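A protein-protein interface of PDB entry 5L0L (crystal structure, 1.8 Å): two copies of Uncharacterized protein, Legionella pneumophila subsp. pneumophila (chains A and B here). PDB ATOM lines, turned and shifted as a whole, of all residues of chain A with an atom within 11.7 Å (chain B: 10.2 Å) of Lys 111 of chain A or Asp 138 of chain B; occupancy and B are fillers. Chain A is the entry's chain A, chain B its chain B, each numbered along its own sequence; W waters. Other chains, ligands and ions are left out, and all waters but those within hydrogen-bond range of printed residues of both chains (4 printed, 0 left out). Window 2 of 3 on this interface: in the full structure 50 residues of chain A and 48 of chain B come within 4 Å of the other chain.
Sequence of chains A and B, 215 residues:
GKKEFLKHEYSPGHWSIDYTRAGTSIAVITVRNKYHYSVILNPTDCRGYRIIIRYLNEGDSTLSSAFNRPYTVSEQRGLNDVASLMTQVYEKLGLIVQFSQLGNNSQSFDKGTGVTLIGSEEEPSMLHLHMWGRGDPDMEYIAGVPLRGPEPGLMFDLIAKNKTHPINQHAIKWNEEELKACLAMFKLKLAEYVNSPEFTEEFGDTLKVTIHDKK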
ATOM      1  N   GLY A   1     -13.107   8.706 -16.445  1.00  0.00           N
ATOM      2  CA  GLY A   1     -13.968   9.650 -17.241  1.00  0.00           C
ATOM      3  C   GLY A   1     -15.477   9.605 -16.949  1.00  0.00           C
ATOM      4  O   GLY A   1     -16.294   9.471 -17.871  1.00  0.00           O
ATOM      5  N   LYS A   2     -15.854   9.733 -15.675  1.00  0.00           N
ATOM      6  CA  LYS A   2     -17.257   9.669 -15.269  1.00  0.00           C
ATOM      7  C   LYS A   2     -17.976  10.984 -15.583  1.00  0.00           C
ATOM      8  O   LYS A   2     -19.149  10.957 -15.904  1.00  0.00           O
ATOM      9  CB  LYS A   2     -17.392   9.342 -13.778  1.00  0.00           C
ATOM     10  CG  LYS A   2     -16.922   7.945 -13.389  1.00  0.00           C
ATOM     11  CD  LYS A   2     -17.884   6.820 -13.782  1.00  0.00           C
ATOM     12  CE  LYS A   2     -19.246   6.959 -13.089  1.00  0.00           C
ATOM     13  NZ  LYS A   2     -20.193   5.857 -13.417  1.00  0.00           N
ATOM     14  N   GLN A 107     -27.345  19.492 -17.817  1.00  0.00           N
ATOM     15  CA  GLN A 107     -26.669  18.286 -17.320  1.00  0.00           C
ATOM     16  C   GLN A 107     -27.489  17.053 -17.689  1.00  0.00           C
ATOM     17  O   GLN A 107     -28.713  17.086 -17.647  1.00  0.00           O
ATOM     18  CB  GLN A 107     -26.469  18.359 -15.807  1.00  0.00           C
ATOM     19  CG  GLN A 107     -25.494  19.451 -15.366  1.00  0.00           C
ATOM     20  CD  GLN A 107     -25.618  19.862 -13.923  1.00  0.00           C
ATOM     21  OE1 GLN A 107     -26.270  19.199 -13.111  1.00  0.00           O
ATOM     22  NE2 GLN A 107     -25.033  21.009 -13.595  1.00  0.00           N
ATOM     23  N   SER A 108     -26.824  15.957 -18.091  1.00  0.00           N
ATOM     24  CA  SER A 108     -27.545  14.747 -18.467  1.00  0.00           C
ATOM     25  C   SER A 108     -26.728  13.504 -18.038  1.00  0.00           C
ATOM     26  O   SER A 108     -25.593  13.623 -17.596  1.00  0.00           O
ATOM     27  CB  SER A 108     -27.855  14.739 -19.974  1.00  0.00           C
ATOM     28  OG  SER A 108     -26.633  14.757 -20.690  1.00  0.00           O
ATOM     29  N   PHE A 109     -27.371  12.348 -18.084  1.00  0.00           N
ATOM     30  CA  PHE A 109     -26.795  11.120 -17.614  1.00  0.00           C
ATOM     31  C   PHE A 109     -27.103   9.997 -18.612  1.00  0.00           C
ATOM     32  O   PHE A 109     -28.217   9.894 -19.091  1.00  0.00           O
ATOM     33  CB  PHE A 109     -27.354  10.761 -16.237  1.00  0.00           C
ATOM     34  CG  PHE A 109     -26.678   9.601 -15.598  1.00  0.00           C
ATOM     35  CD1 PHE A 109     -25.351   9.689 -15.194  1.00  0.00           C
ATOM     36  CD2 PHE A 109     -27.360   8.414 -15.406  1.00  0.00           C
ATOM     37  CE1 PHE A 109     -24.711   8.609 -14.610  1.00  0.00           C
ATOM     38  CE2 PHE A 109     -26.724   7.329 -14.800  1.00  0.00           C
ATOM     39  CZ  PHE A 109     -25.392   7.426 -14.414  1.00  0.00           C
ATOM     40  N   ASP A 110     -26.098   9.178 -18.894  1.00  0.00           N
ATOM     41  CA  ASP A 110     -26.246   7.995 -19.747  1.00  0.00           C
ATOM     42  C   ASP A 110     -26.057   6.785 -18.837  1.00  0.00           C
ATOM     43  O   ASP A 110     -24.975   6.500 -18.392  1.00  0.00           O
ATOM     44  CB  ASP A 110     -25.243   8.035 -20.898  1.00  0.00           C
ATOM     45  CG  ASP A 110     -25.385   6.838 -21.858  1.00  0.00           C
ATOM     46  OD1 ASP A 110     -25.731   5.744 -21.405  1.00  0.00           O
ATOM     47  OD2 ASP A 110     -25.078   6.989 -23.057  1.00  0.00           O
ATOM     48  N   LYS A 111     -27.162   6.133 -18.518  1.00  0.00           N
ATOM     49  CA  LYS A 111     -27.180   4.999 -17.611  1.00  0.00           C
ATOM     50  C   LYS A 111     -26.304   3.856 -18.130  1.00  0.00           C
ATOM     51  O   LYS A 111     -25.585   3.234 -17.357  1.00  0.00           O
ATOM     52  CB  LYS A 111     -28.627   4.525 -17.436  1.00  0.00           C
ATOM     53  CG  LYS A 111     -28.809   3.286 -16.575  1.00  0.00           C
ATOM     54  CD  LYS A 111     -28.246   3.451 -15.166  1.00  0.00           C
ATOM     55  CE  LYS A 111     -29.040   2.599 -14.196  1.00  0.00           C
ATOM     56  NZ  LYS A 111     -28.453   2.649 -12.828  1.00  0.00           N
ATOM     57  N   GLY A 112     -26.362   3.609 -19.437  1.00  0.00           N
ATOM     58  CA  GLY A 112     -25.526   2.576 -20.083  1.00  0.00           C
ATOM     59  C   GLY A 112     -24.039   2.720 -19.817  1.00  0.00           C
ATOM     60  O   GLY A 112     -23.367   1.749 -19.489  1.00  0.00           O
ATOM     61  N   THR A 113     -23.516   3.935 -19.944  1.00  0.00           N
ATOM     62  CA  THR A 113     -22.087   4.186 -19.775  1.00  0.00           C
ATOM     63  C   THR A 113     -21.712   4.715 -18.395  1.00  0.00           C
ATOM     64  O   THR A 113     -20.538   4.743 -18.042  1.00  0.00           O
ATOM     65  CB  THR A 113     -21.608   5.187 -20.838  1.00  0.00           C
ATOM     66  OG1 THR A 113     -22.265   6.443 -20.637  1.00  0.00           O
ATOM     67  CG2 THR A 113     -21.929   4.663 -22.227  1.00  0.00           C
ATOM     68  N   GLY A 114     -22.696   5.182 -17.633  1.00  0.00           N
ATOM     69  CA  GLY A 114     -22.441   5.834 -16.357  1.00  0.00           C
ATOM     70  C   GLY A 114     -21.812   7.224 -16.441  1.00  0.00           C
ATOM     71  O   GLY A 114     -21.244   7.705 -15.456  1.00  0.00           O
ATOM     72  N   VAL A 115     -21.916   7.873 -17.600  1.00  0.00           N
ATOM     73  CA  VAL A 115     -21.265   9.142 -17.829  1.00  0.00           C
ATOM     74  C   VAL A 115     -22.266  10.298 -17.601  1.00  0.00           C
ATOM     75  O   VAL A 115     -23.408  10.256 -18.078  1.00  0.00           O
ATOM     76  CB  VAL A 115     -20.679   9.223 -19.258  1.00  0.00           C
ATOM     77  CG1 VAL A 115     -20.136  10.613 -19.567  1.00  0.00           C
ATOM     78  CG2 VAL A 115     -19.590   8.167 -19.464  1.00  0.00           C
ATOM     79  N   THR A 116     -21.803  11.293 -16.847  1.00  0.00           N
ATOM     80  CA  THR A 116     -22.520  12.537 -16.623  1.00  0.00           C
ATOM     81  C   THR A 116     -21.961  13.563 -17.626  1.00  0.00           C
ATOM     82  O   THR A 116     -20.747  13.822 -17.646  1.00  0.00           O
ATOM     83  CB  THR A 116     -22.315  13.031 -15.181  1.00  0.00           C
ATOM     84  OG1 THR A 116     -22.857  12.086 -14.244  1.00  0.00           O
ATOM     85  CG2 THR A 116     -22.970  14.374 -14.972  1.00  0.00           C
ATOM     86  N   LEU A 117     -22.831  14.116 -18.470  1.00  0.00           N
ATOM     87  CA  LEU A 117     -22.428  15.039 -19.515  1.00  0.00           C
ATOM     88  C   LEU A 117     -22.832  16.473 -19.122  1.00  0.00           C
ATOM     89  O   LEU A 117     -23.976  16.683 -18.728  1.00  0.00           O
ATOM     90  CB  LEU A 117     -23.128  14.668 -20.818  1.00  0.00           C
ATOM     91  CG  LEU A 117     -22.799  15.512 -22.058  1.00  0.00           C
ATOM     92  CD1 LEU A 117     -21.303  15.448 -22.346  1.00  0.00           C
ATOM     93  CD2 LEU A 117     -23.626  15.080 -23.260  1.00  0.00           C
ATOM     94  N   ASN A 162     -36.273  18.169 -17.645  1.00  0.00           N
ATOM     95  CA  ASN A 162     -36.374  16.720 -17.482  1.00  0.00           C
ATOM     96  C   ASN A 162     -37.102  16.402 -16.156  1.00  0.00           C
ATOM     97  O   ASN A 162     -36.647  16.760 -15.068  1.00  0.00           O
ATOM     98  CB  ASN A 162     -34.955  16.144 -17.515  1.00  0.00           C
ATOM     99  CG  ASN A 162     -34.907  14.633 -17.585  1.00  0.00           C
ATOM    100  OD1 ASN A 162     -35.936  13.956 -17.572  1.00  0.00           O
ATOM    101  ND2 ASN A 162     -33.685  14.086 -17.643  1.00  0.00           N
ATOM    102  N   GLY B  48     -26.472  12.523  -2.132  1.00  0.00           N
ATOM    103  CA  GLY B  48     -25.576  13.557  -2.636  1.00  0.00           C
ATOM    104  C   GLY B  48     -24.489  14.020  -1.684  1.00  0.00           C
ATOM    105  O   GLY B  48     -23.882  15.054  -1.945  1.00  0.00           O
ATOM    106  N   TYR B  49     -24.246  13.272  -0.599  1.00  0.00           N
ATOM    107  CA  TYR B  49     -23.372  13.691   0.491  1.00  0.00           C
ATOM    108  C   TYR B  49     -23.718  15.125   0.949  1.00  0.00           C
ATOM    109  O   TYR B  49     -22.843  15.966   1.122  1.00  0.00           O
ATOM    110  CB  TYR B  49     -21.889  13.644   0.082  1.00  0.00           C
ATOM    111  CG  TYR B  49     -21.416  12.377  -0.611  1.00  0.00           C
ATOM    112  CD1 TYR B  49     -21.967  11.113  -0.326  1.00  0.00           C
ATOM    113  CD2 TYR B  49     -20.391  12.447  -1.540  1.00  0.00           C
ATOM    114  CE1 TYR B  49     -21.516   9.964  -0.967  1.00  0.00           C
ATOM    115  CE2 TYR B  49     -19.907  11.305  -2.176  1.00  0.00           C
ATOM    116  CZ  TYR B  49     -20.456  10.073  -1.896  1.00  0.00           C
ATOM    117  OH  TYR B  49     -19.981   8.960  -2.556  1.00  0.00           O
ATOM    118  N   LEU B  95     -17.533  15.611  -8.382  1.00  0.00           N
ATOM    119  CA  LEU B  95     -18.976  15.803  -8.353  1.00  0.00           C
ATOM    120  C   LEU B  95     -19.366  17.157  -8.953  1.00  0.00           C
ATOM    121  O   LEU B  95     -18.605  18.112  -8.887  1.00  0.00           O
ATOM    122  CB  LEU B  95     -19.478  15.694  -6.906  1.00  0.00           C
ATOM    123  CG  LEU B  95     -19.362  14.285  -6.289  1.00  0.00           C
ATOM    124  CD1 LEU B  95     -19.586  14.319  -4.782  1.00  0.00           C
ATOM    125  CD2 LEU B  95     -20.288  13.319  -6.990  1.00  0.00           C
ATOM    126  N   GLY B 133     -23.688  17.009  -4.003  1.00  0.00           N
ATOM    127  CA  GLY B 133     -23.077  16.636  -5.262  1.00  0.00           C
ATOM    128  C   GLY B 133     -23.966  15.810  -6.180  1.00  0.00           C
ATOM    129  O   GLY B 133     -24.828  15.079  -5.708  1.00  0.00           O
ATOM    130  N   ARG B 134     -23.787  15.984  -7.493  1.00  0.00           N
ATOM    131  CA  ARG B 134     -24.499  15.209  -8.514  1.00  0.00           C
ATOM    132  C   ARG B 134     -23.513  14.404  -9.375  1.00  0.00           C
ATOM    133  O   ARG B 134     -22.385  14.827  -9.658  1.00  0.00           O
ATOM    134  CB  ARG B 134     -25.359  16.104  -9.411  1.00  0.00           C
ATOM    135  CG  ARG B 134     -26.344  17.029  -8.662  1.00  0.00           C
ATOM    136  CD  ARG B 134     -27.381  16.258  -7.852  1.00  0.00           C
ATOM    137  NE  ARG B 134     -28.245  15.444  -8.716  1.00  0.00           N
ATOM    138  CZ  ARG B 134     -29.276  15.908  -9.434  1.00  0.00           C
ATOM    139  NH1 ARG B 134     -29.930  15.069 -10.225  1.00  0.00           N
ATOM    140  NH2 ARG B 134     -29.676  17.186  -9.387  1.00  0.00           N
ATOM    141  N   GLY B 135     -23.988  13.249  -9.805  1.00  0.00           N
ATOM    142  CA  GLY B 135     -23.176  12.318 -10.570  1.00  0.00           C
ATOM    143  C   GLY B 135     -23.928  10.997 -10.680  1.00  0.00           C
ATOM    144  O   GLY B 135     -25.136  10.956 -10.471  1.00  0.00           O
ATOM    145  N   ASP B 136     -23.208   9.906 -10.950  1.00  0.00           N
ATOM    146  CA  ASP B 136     -23.837   8.576 -11.050  1.00  0.00           C
ATOM    147  C   ASP B 136     -24.304   8.165  -9.648  1.00  0.00           C
ATOM    148  O   ASP B 136     -23.469   7.973  -8.775  1.00  0.00           O
ATOM    149  CB  ASP B 136     -22.792   7.584 -11.584  1.00  0.00           C
ATOM    150  CG  ASP B 136     -23.275   6.155 -11.660  1.00  0.00           C
ATOM    151  OD1 ASP B 136     -24.351   5.784 -11.149  1.00  0.00           O
ATOM    152  OD2 ASP B 136     -22.483   5.353 -12.235  1.00  0.00           O
ATOM    153  N   PRO B 137     -25.624   8.007  -9.437  1.00  0.00           N
ATOM    154  CA  PRO B 137     -26.084   7.713  -8.075  1.00  0.00           C
ATOM    155  C   PRO B 137     -25.558   6.406  -7.476  1.00  0.00           C
ATOM    156  O   PRO B 137     -25.545   6.255  -6.244  1.00  0.00           O
ATOM    157  CB  PRO B 137     -27.623   7.622  -8.237  1.00  0.00           C
ATOM    158  CG  PRO B 137     -27.910   8.479  -9.423  1.00  0.00           C
ATOM    159  CD  PRO B 137     -26.765   8.195 -10.359  1.00  0.00           C
ATOM    160  N   ASP B 138     -25.162   5.467  -8.342  1.00  0.00           N
ATOM    161  CA  ASP B 138     -24.632   4.177  -7.893  1.00  0.00           C
ATOM    162  C   ASP B 138     -23.118   4.171  -7.664  1.00  0.00           C
ATOM    163  O   ASP B 138     -22.604   3.191  -7.126  1.00  0.00           O
ATOM    164  CB  ASP B 138     -24.997   3.073  -8.903  1.00  0.00           C
ATOM    165  CG  ASP B 138     -26.501   2.770  -8.935  1.00  0.00           C
ATOM    166  OD1 ASP B 138     -27.236   3.000  -7.943  1.00  0.00           O
ATOM    167  OD2 ASP B 138     -26.954   2.292  -9.991  1.00  0.00           O
ATOM    168  N   MET B 139     -22.422   5.242  -8.056  1.00  0.00           N
ATOM    169  CA  MET B 139     -20.970   5.300  -7.948  1.00  0.00           C
ATOM    170  C   MET B 139     -20.574   5.670  -6.536  1.00  0.00           C
ATOM    171  O   MET B 139     -21.099   6.618  -5.952  1.00  0.00           O
ATOM    172  CB  MET B 139     -20.439   6.253  -8.996  1.00  0.00           C
ATOM    173  CG  MET B 139     -19.003   6.690  -8.853  1.00  0.00           C
ATOM    174  SD  MET B 139     -17.792   5.201  -9.250  1.00  0.00           S
ATOM    175  CE  MET B 139     -16.174   6.320  -9.183  1.00  0.00           C
ATOM    176  N   GLU B 140     -19.629   4.911  -5.977  1.00  0.00           N
ATOM    177  CA  GLU B 140     -19.024   5.261  -4.689  1.00  0.00           C
ATOM    178  C   GLU B 140     -17.880   6.261  -4.893  1.00  0.00           C
ATOM    179  O   GLU B 140     -16.698   5.887  -4.896  1.00  0.00           O
ATOM    180  CB  GLU B 140     -18.560   3.983  -3.945  1.00  0.00           C
ATOM    181  CG  GLU B 140     -19.693   3.014  -3.698  1.00  0.00           C
ATOM    182  CD  GLU B 140     -19.278   1.755  -2.955  1.00  0.00           C
ATOM    183  OE1 GLU B 140     -18.075   1.554  -2.672  1.00  0.00           O
ATOM    184  OE2 GLU B 140     -20.196   0.992  -2.631  1.00  0.00           O
ATOM    185  N   TYR B 141     -18.224   7.540  -5.076  1.00  0.00           N
ATOM    186  CA  TYR B 141     -17.228   8.628  -5.186  1.00  0.00           C
ATOM    187  C   TYR B 141     -16.319   8.700  -3.939  1.00  0.00           C
ATOM    188  O   TYR B 141     -15.150   9.102  -4.024  1.00  0.00           O
ATOM    189  CB  TYR B 141     -17.925   9.970  -5.418  1.00  0.00           C
ATOM    190  CG  TYR B 141     -18.579  10.056  -6.784  1.00  0.00           C
ATOM    191  CD1 TYR B 141     -17.881  10.537  -7.880  1.00  0.00           C
ATOM    192  CD2 TYR B 141     -19.889   9.634  -6.990  1.00  0.00           C
ATOM    193  CE1 TYR B 141     -18.478  10.626  -9.144  1.00  0.00           C
ATOM    194  CE2 TYR B 141     -20.493   9.713  -8.243  1.00  0.00           C
ATOM    195  CZ  TYR B 141     -19.781  10.188  -9.317  1.00  0.00           C
ATOM    196  OH  TYR B 141     -20.358  10.244 -10.556  1.00  0.00           O
ATOM    197  N   ILE B 142     -16.885   8.318  -2.798  1.00  0.00           N
ATOM    198  CA  ILE B 142     -16.152   7.985  -1.584  1.00  0.00           C
ATOM    199  C   ILE B 142     -16.316   6.483  -1.379  1.00  0.00           C
ATOM    200  O   ILE B 142     -17.455   5.974  -1.332  1.00  0.00           O
ATOM    201  CB  ILE B 142     -16.711   8.770  -0.379  1.00  0.00           C
ATOM    202  CG1 ILE B 142     -16.582  10.275  -0.630  1.00  0.00           C
ATOM    203  CG2 ILE B 142     -16.046   8.342   0.916  1.00  0.00           C
ATOM    204  CD1 ILE B 142     -17.293  11.150   0.356  1.00  0.00           C
ATOM    205  N   ALA B 143     -15.202   5.748  -1.279  1.00  0.00           N
ATOM    206  CA  ALA B 143     -15.305   4.286  -1.177  1.00  0.00           C
ATOM    207  C   ALA B 143     -16.223   3.841  -0.009  1.00  0.00           C
ATOM    208  O   ALA B 143     -16.171   4.378   1.085  1.00  0.00           O
ATOM    209  CB  ALA B 143     -13.928   3.616  -1.081  1.00  0.00           C
ATOM    210  N   GLY B 144     -17.103   2.910  -0.299  1.00  0.00           N
ATOM    211  CA  GLY B 144     -18.087   2.419   0.662  1.00  0.00           C
ATOM    212  C   GLY B 144     -19.359   3.217   0.753  1.00  0.00           C
ATOM    213  O   GLY B 144     -20.242   2.823   1.511  1.00  0.00           O
ATOM    214  N   VAL B 145     -19.487   4.315  -0.020  1.00  0.00           N
ATOM    215  CA  VAL B 145     -20.657   5.200   0.089  1.00  0.00           C
ATOM    216  C   VAL B 145     -21.202   5.593  -1.279  1.00  0.00           C
ATOM    217  O   VAL B 145     -20.683   6.491  -1.941  1.00  0.00           O
ATOM    218  CB  VAL B 145     -20.396   6.476   0.896  1.00  0.00           C
ATOM    219  CG1 VAL B 145     -21.731   7.115   1.284  1.00  0.00           C
ATOM    220  CG2 VAL B 145     -19.546   6.186   2.132  1.00  0.00           C
ATOM    221  N   PRO B 146     -22.265   4.913  -1.722  1.00  0.00           N
ATOM    222  CA  PRO B 146     -22.840   5.325  -2.995  1.00  0.00           C
ATOM    223  C   PRO B 146     -23.375   6.775  -2.906  1.00  0.00           C
ATOM    224  O   PRO B 146     -23.890   7.143  -1.872  1.00  0.00           O
ATOM    225  CB  PRO B 146     -24.019   4.367  -3.209  1.00  0.00           C
ATOM    226  CG  PRO B 146     -23.971   3.372  -2.111  1.00  0.00           C
ATOM    227  CD  PRO B 146     -22.934   3.761  -1.104  1.00  0.00           C
ATOM    228  N   LEU B 147     -23.254   7.543  -3.980  1.00  0.00           N
ATOM    229  CA  LEU B 147     -23.687   8.934  -3.960  1.00  0.00           C
ATOM    230  C   LEU B 147     -25.169   9.071  -3.615  1.00  0.00           C
ATOM    231  O   LEU B 147     -25.543   9.923  -2.809  1.00  0.00           O
ATOM    232  CB  LEU B 147     -23.448   9.604  -5.314  1.00  0.00           C
ATOM    233  CG  LEU B 147     -23.759  11.115  -5.337  1.00  0.00           C
ATOM    234  CD1 LEU B 147     -22.797  11.922  -4.473  1.00  0.00           C
ATOM    235  CD2 LEU B 147     -23.698  11.608  -6.765  1.00  0.00           C
ATOM    236  N   ARG B 148     -25.989   8.256  -4.284  1.00  0.00           N
ATOM    237  CA  ARG B 148     -27.451   8.323  -4.214  1.00  0.00           C
ATOM    238  C   ARG B 148     -27.966   9.679  -4.765  1.00  0.00           C
ATOM    239  O   ARG B 148     -27.188  10.468  -5.321  1.00  0.00           O
ATOM    240  CB  ARG B 148     -27.934   8.036  -2.798  1.00  0.00           C
ATOM    241  CG  ARG B 148     -27.456   6.715  -2.227  1.00  0.00           C
ATOM    242  CD  ARG B 148     -27.973   6.557  -0.814  1.00  0.00           C
ATOM    243  NE  ARG B 148     -27.620   5.249  -0.274  1.00  0.00           N
ATOM    244  CZ  ARG B 148     -26.553   4.974   0.485  1.00  0.00           C
ATOM    245  NH1 ARG B 148     -25.645   5.902   0.861  1.00  0.00           N
ATOM    246  NH2 ARG B 148     -26.382   3.714   0.869  1.00  0.00           N
ATOM    247  N   GLY B 149     -29.262   9.934  -4.636  1.00  0.00           N
ATOM    248  CA  GLY B 149     -29.900  11.057  -5.276  1.00  0.00           C
ATOM    249  C   GLY B 149     -30.341  10.680  -6.686  1.00  0.00           C
ATOM    250  O   GLY B 149     -30.002   9.603  -7.189  1.00  0.00           O
ATOM    251  N   PRO B 150     -31.135  11.546  -7.316  1.00  0.00           N
ATOM    252  CA  PRO B 150     -31.616  11.280  -8.672  1.00  0.00           C
ATOM    253  C   PRO B 150     -30.522  11.464  -9.708  1.00  0.00           C
ATOM    254  O   PRO B 150     -29.553  12.192  -9.466  1.00  0.00           O
ATOM    255  CB  PRO B 150     -32.725  12.303  -8.865  1.00  0.00           C
ATOM    256  CG  PRO B 150     -32.493  13.334  -7.851  1.00  0.00           C
ATOM    257  CD  PRO B 150     -31.637  12.810  -6.765  1.00  0.00           C
ATOM    258  N   GLU B 151     -30.695  10.813 -10.865  1.00  0.00           N
ATOM    259  CA  GLU B 151     -29.748  10.969 -11.956  1.00  0.00           C
ATOM    260  C   GLU B 151     -29.578  12.436 -12.375  1.00  0.00           C
ATOM    261  O   GLU B 151     -30.555  13.180 -12.379  1.00  0.00           O
ATOM    262  CB  GLU B 151     -30.181  10.134 -13.179  1.00  0.00           C
ATOM    263  CG  GLU B 151     -29.977   8.635 -12.923  1.00  0.00           C
ATOM    264  CD  GLU B 151     -30.451   7.759 -14.077  1.00  0.00           C
ATOM    265  OE1 GLU B 151     -30.944   8.337 -15.056  1.00  0.00           O
ATOM    266  OE2 GLU B 151     -30.287   6.510 -13.995  1.00  0.00           O
ATOM    267  N   PRO B 152     -28.354  12.839 -12.752  1.00  0.00           N
ATOM    268  CA  PRO B 152     -28.132  14.182 -13.302  1.00  0.00           C
ATOM    269  C   PRO B 152     -29.109  14.542 -14.413  1.00  0.00           C
ATOM    270  O   PRO B 152     -29.472  13.671 -15.214  1.00  0.00           O
ATOM    271  CB  PRO B 152     -26.713  14.119 -13.843  1.00  0.00           C
ATOM    272  CG  PRO B 152     -26.054  13.125 -12.959  1.00  0.00           C
ATOM    273  CD  PRO B 152     -27.101  12.078 -12.702  1.00  0.00           C
ATOM    274  N   ILE B 172     -32.804   9.887   2.899  1.00  0.00           N
ATOM    275  CA  ILE B 172     -32.251   8.576   3.267  1.00  0.00           C
ATOM    276  C   ILE B 172     -31.348   8.771   4.481  1.00  0.00           C
ATOM    277  O   ILE B 172     -30.340   9.450   4.395  1.00  0.00           O
ATOM    278  CB  ILE B 172     -31.513   7.924   2.096  1.00  0.00           C
ATOM    279  CG1 ILE B 172     -32.503   7.708   0.934  1.00  0.00           C
ATOM    280  CG2 ILE B 172     -30.843   6.606   2.541  1.00  0.00           C
ATOM    281  CD1 ILE B 172     -31.913   7.129  -0.349  1.00  0.00           C
ATOM    282  N   GLU B 178     -21.160   4.067   6.790  1.00  0.00           N
ATOM    283  CA  GLU B 178     -21.075   5.009   5.672  1.00  0.00           C
ATOM    284  C   GLU B 178     -20.812   6.433   6.154  1.00  0.00           C
ATOM    285  O   GLU B 178     -19.981   7.149   5.557  1.00  0.00           O
ATOM    286  CB  GLU B 178     -22.313   4.953   4.789  1.00  0.00           C
ATOM    287  CG  GLU B 178     -22.437   3.625   4.081  1.00  0.00           C
ATOM    288  CD  GLU B 178     -23.603   3.540   3.136  1.00  0.00           C
ATOM    289  OE1 GLU B 178     -24.201   4.588   2.790  1.00  0.00           O
ATOM    290  OE2 GLU B 178     -23.937   2.382   2.774  1.00  0.00           O
HETATM  291  O   HOH W   1     -28.991   5.505 -11.750  1.00  0.00           O
HETATM  292  O   HOH W   2     -21.166   9.968 -13.785  1.00  0.00           O
HETATM  293  O   HOH W   3     -31.387  12.360 -16.447  1.00  0.00           O
HETATM  294  O   HOH W   4     -28.265  17.464 -12.515  1.00  0.00           O
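NZ of Lys 2 of chain A lies within salt-bridge range of OD2 of Asp 136 of chain B, at 2.6 Å.
The side-chain amino group (NZ) of Lys 111 of chain A lies within salt-bridge range of the side-chain carboxylate (OD2) of Asp 138 of chain B (3.2 Å).
The backbone NH (N) of Leu 117 of chain A is in hydrogen-bond range of the backbone carbonyl oxygen (O) of Ser 108 of chain A (2.9 Å).
The backbone NH (N) of Thr 116 of chain A lies within hydrogen-bond range of the backbone carbonyl oxygen (O) of Lys 2 of chain A (2.8 Å).
The backbone NH (N) of Asp 136 of chain B sits at hydrogen-bond distance from the side-chain hydroxyl (OH) of Tyr 141 of chain B, 2.9 Å away.
The backbone carbonyl oxygen (O) of Glu 151 of chain B is in hydrogen-bond range of the guanidinium group (NH1) of Arg 134 of chain B (2.9 Å).
The side-chain amino group (NZ) of Lys 2 of chain A sits at hydrogen-bond distance from the backbone carbonyl oxygen (O) of Gly 114 of chain A (2.9 Å).
The backbone NH (N) of Asp 138 of chain B lies within hydrogen-bond range of the side-chain carboxylate (OD1) of Asp 136 of chain B, 2.9 Å away.
Among the printed residues, pairs that only touch across the chains: Phe 109 of chain A with Glu 151 of chain B, Thr 116 of chain A with Pro 152 of chain B, Phe 109 of chain A with Asp 136 of chain B, Thr 116 of chain A with Gly 135 of chain B, Phe 109 of chain A with Pro 152 of chain B, Lys 111 of chain A with Glu 151 of chain B, Ser 108 of chain A with Pro 152 of chain B and Thr 116 of chain A with Asp 136 of chain B.
Of the printed residues of chain B, Lys 2 of chain A touches Asp 136.
Printed residues of chain B within 4 Å of Ser 108 of chain A: Pro 152 (3.9 Å).
No residue of chain B comes within 4 Å of Asp 110 of chain A.
No residue of chain B comes within 4 Å of Thr 113 of chain A.
Of chain A, only Lys 2, Phe 109 and Thr 116 come within 4 Å of Asp 136 of chain B.
The nearest printed residue of chain A that does not touch Gly 135 of chain B is Phe 109 of chain A (4.7 Å).
Printed residues of chain B that touch a printed residue of chain A: Gly 135, Asp 136, Asp 138, Glu 151 and Pro 152.
Along chain B the printed residues that touch a printed residue of chain A span positions 135 to 152.
Hydrophobic or aromatic side chains of chain A within 4 Å of the printed part of chain B: Phe 109.
Along chain A the printed residues that touch a printed residue of chain B span positions 2 to 116.
No position is printed for both chains.
Water W3 lies within hydrogen-bond range of the backbone carbonyl oxygen of Pro 152 of chain B and the side-chain amide nitrogen of Asn 162 of chain A.
Water W4 bridges the side-chain amide oxygen of Gln 107 of chain A and the guanidinium group of Arg 134 of chain B.
Water W2 lies within hydrogen-bond range of the side-chain hydroxyl (OG1) of Thr 116 of chain A, the backbone carbonyl oxygen (O) of Gly 114 of chain A, the backbone carbonyl oxygen (O) of Lys 2 of chain A, the side-chain hydroxyl (OH) of Tyr 141 of chain B and the backbone NH (N) of Asp 136 of chain B.
Water W1 bridges the side-chain carboxylate (OE2) of Glu 151 of chain B and the side-chain amino group (NZ) of Lys 111 of chain A.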
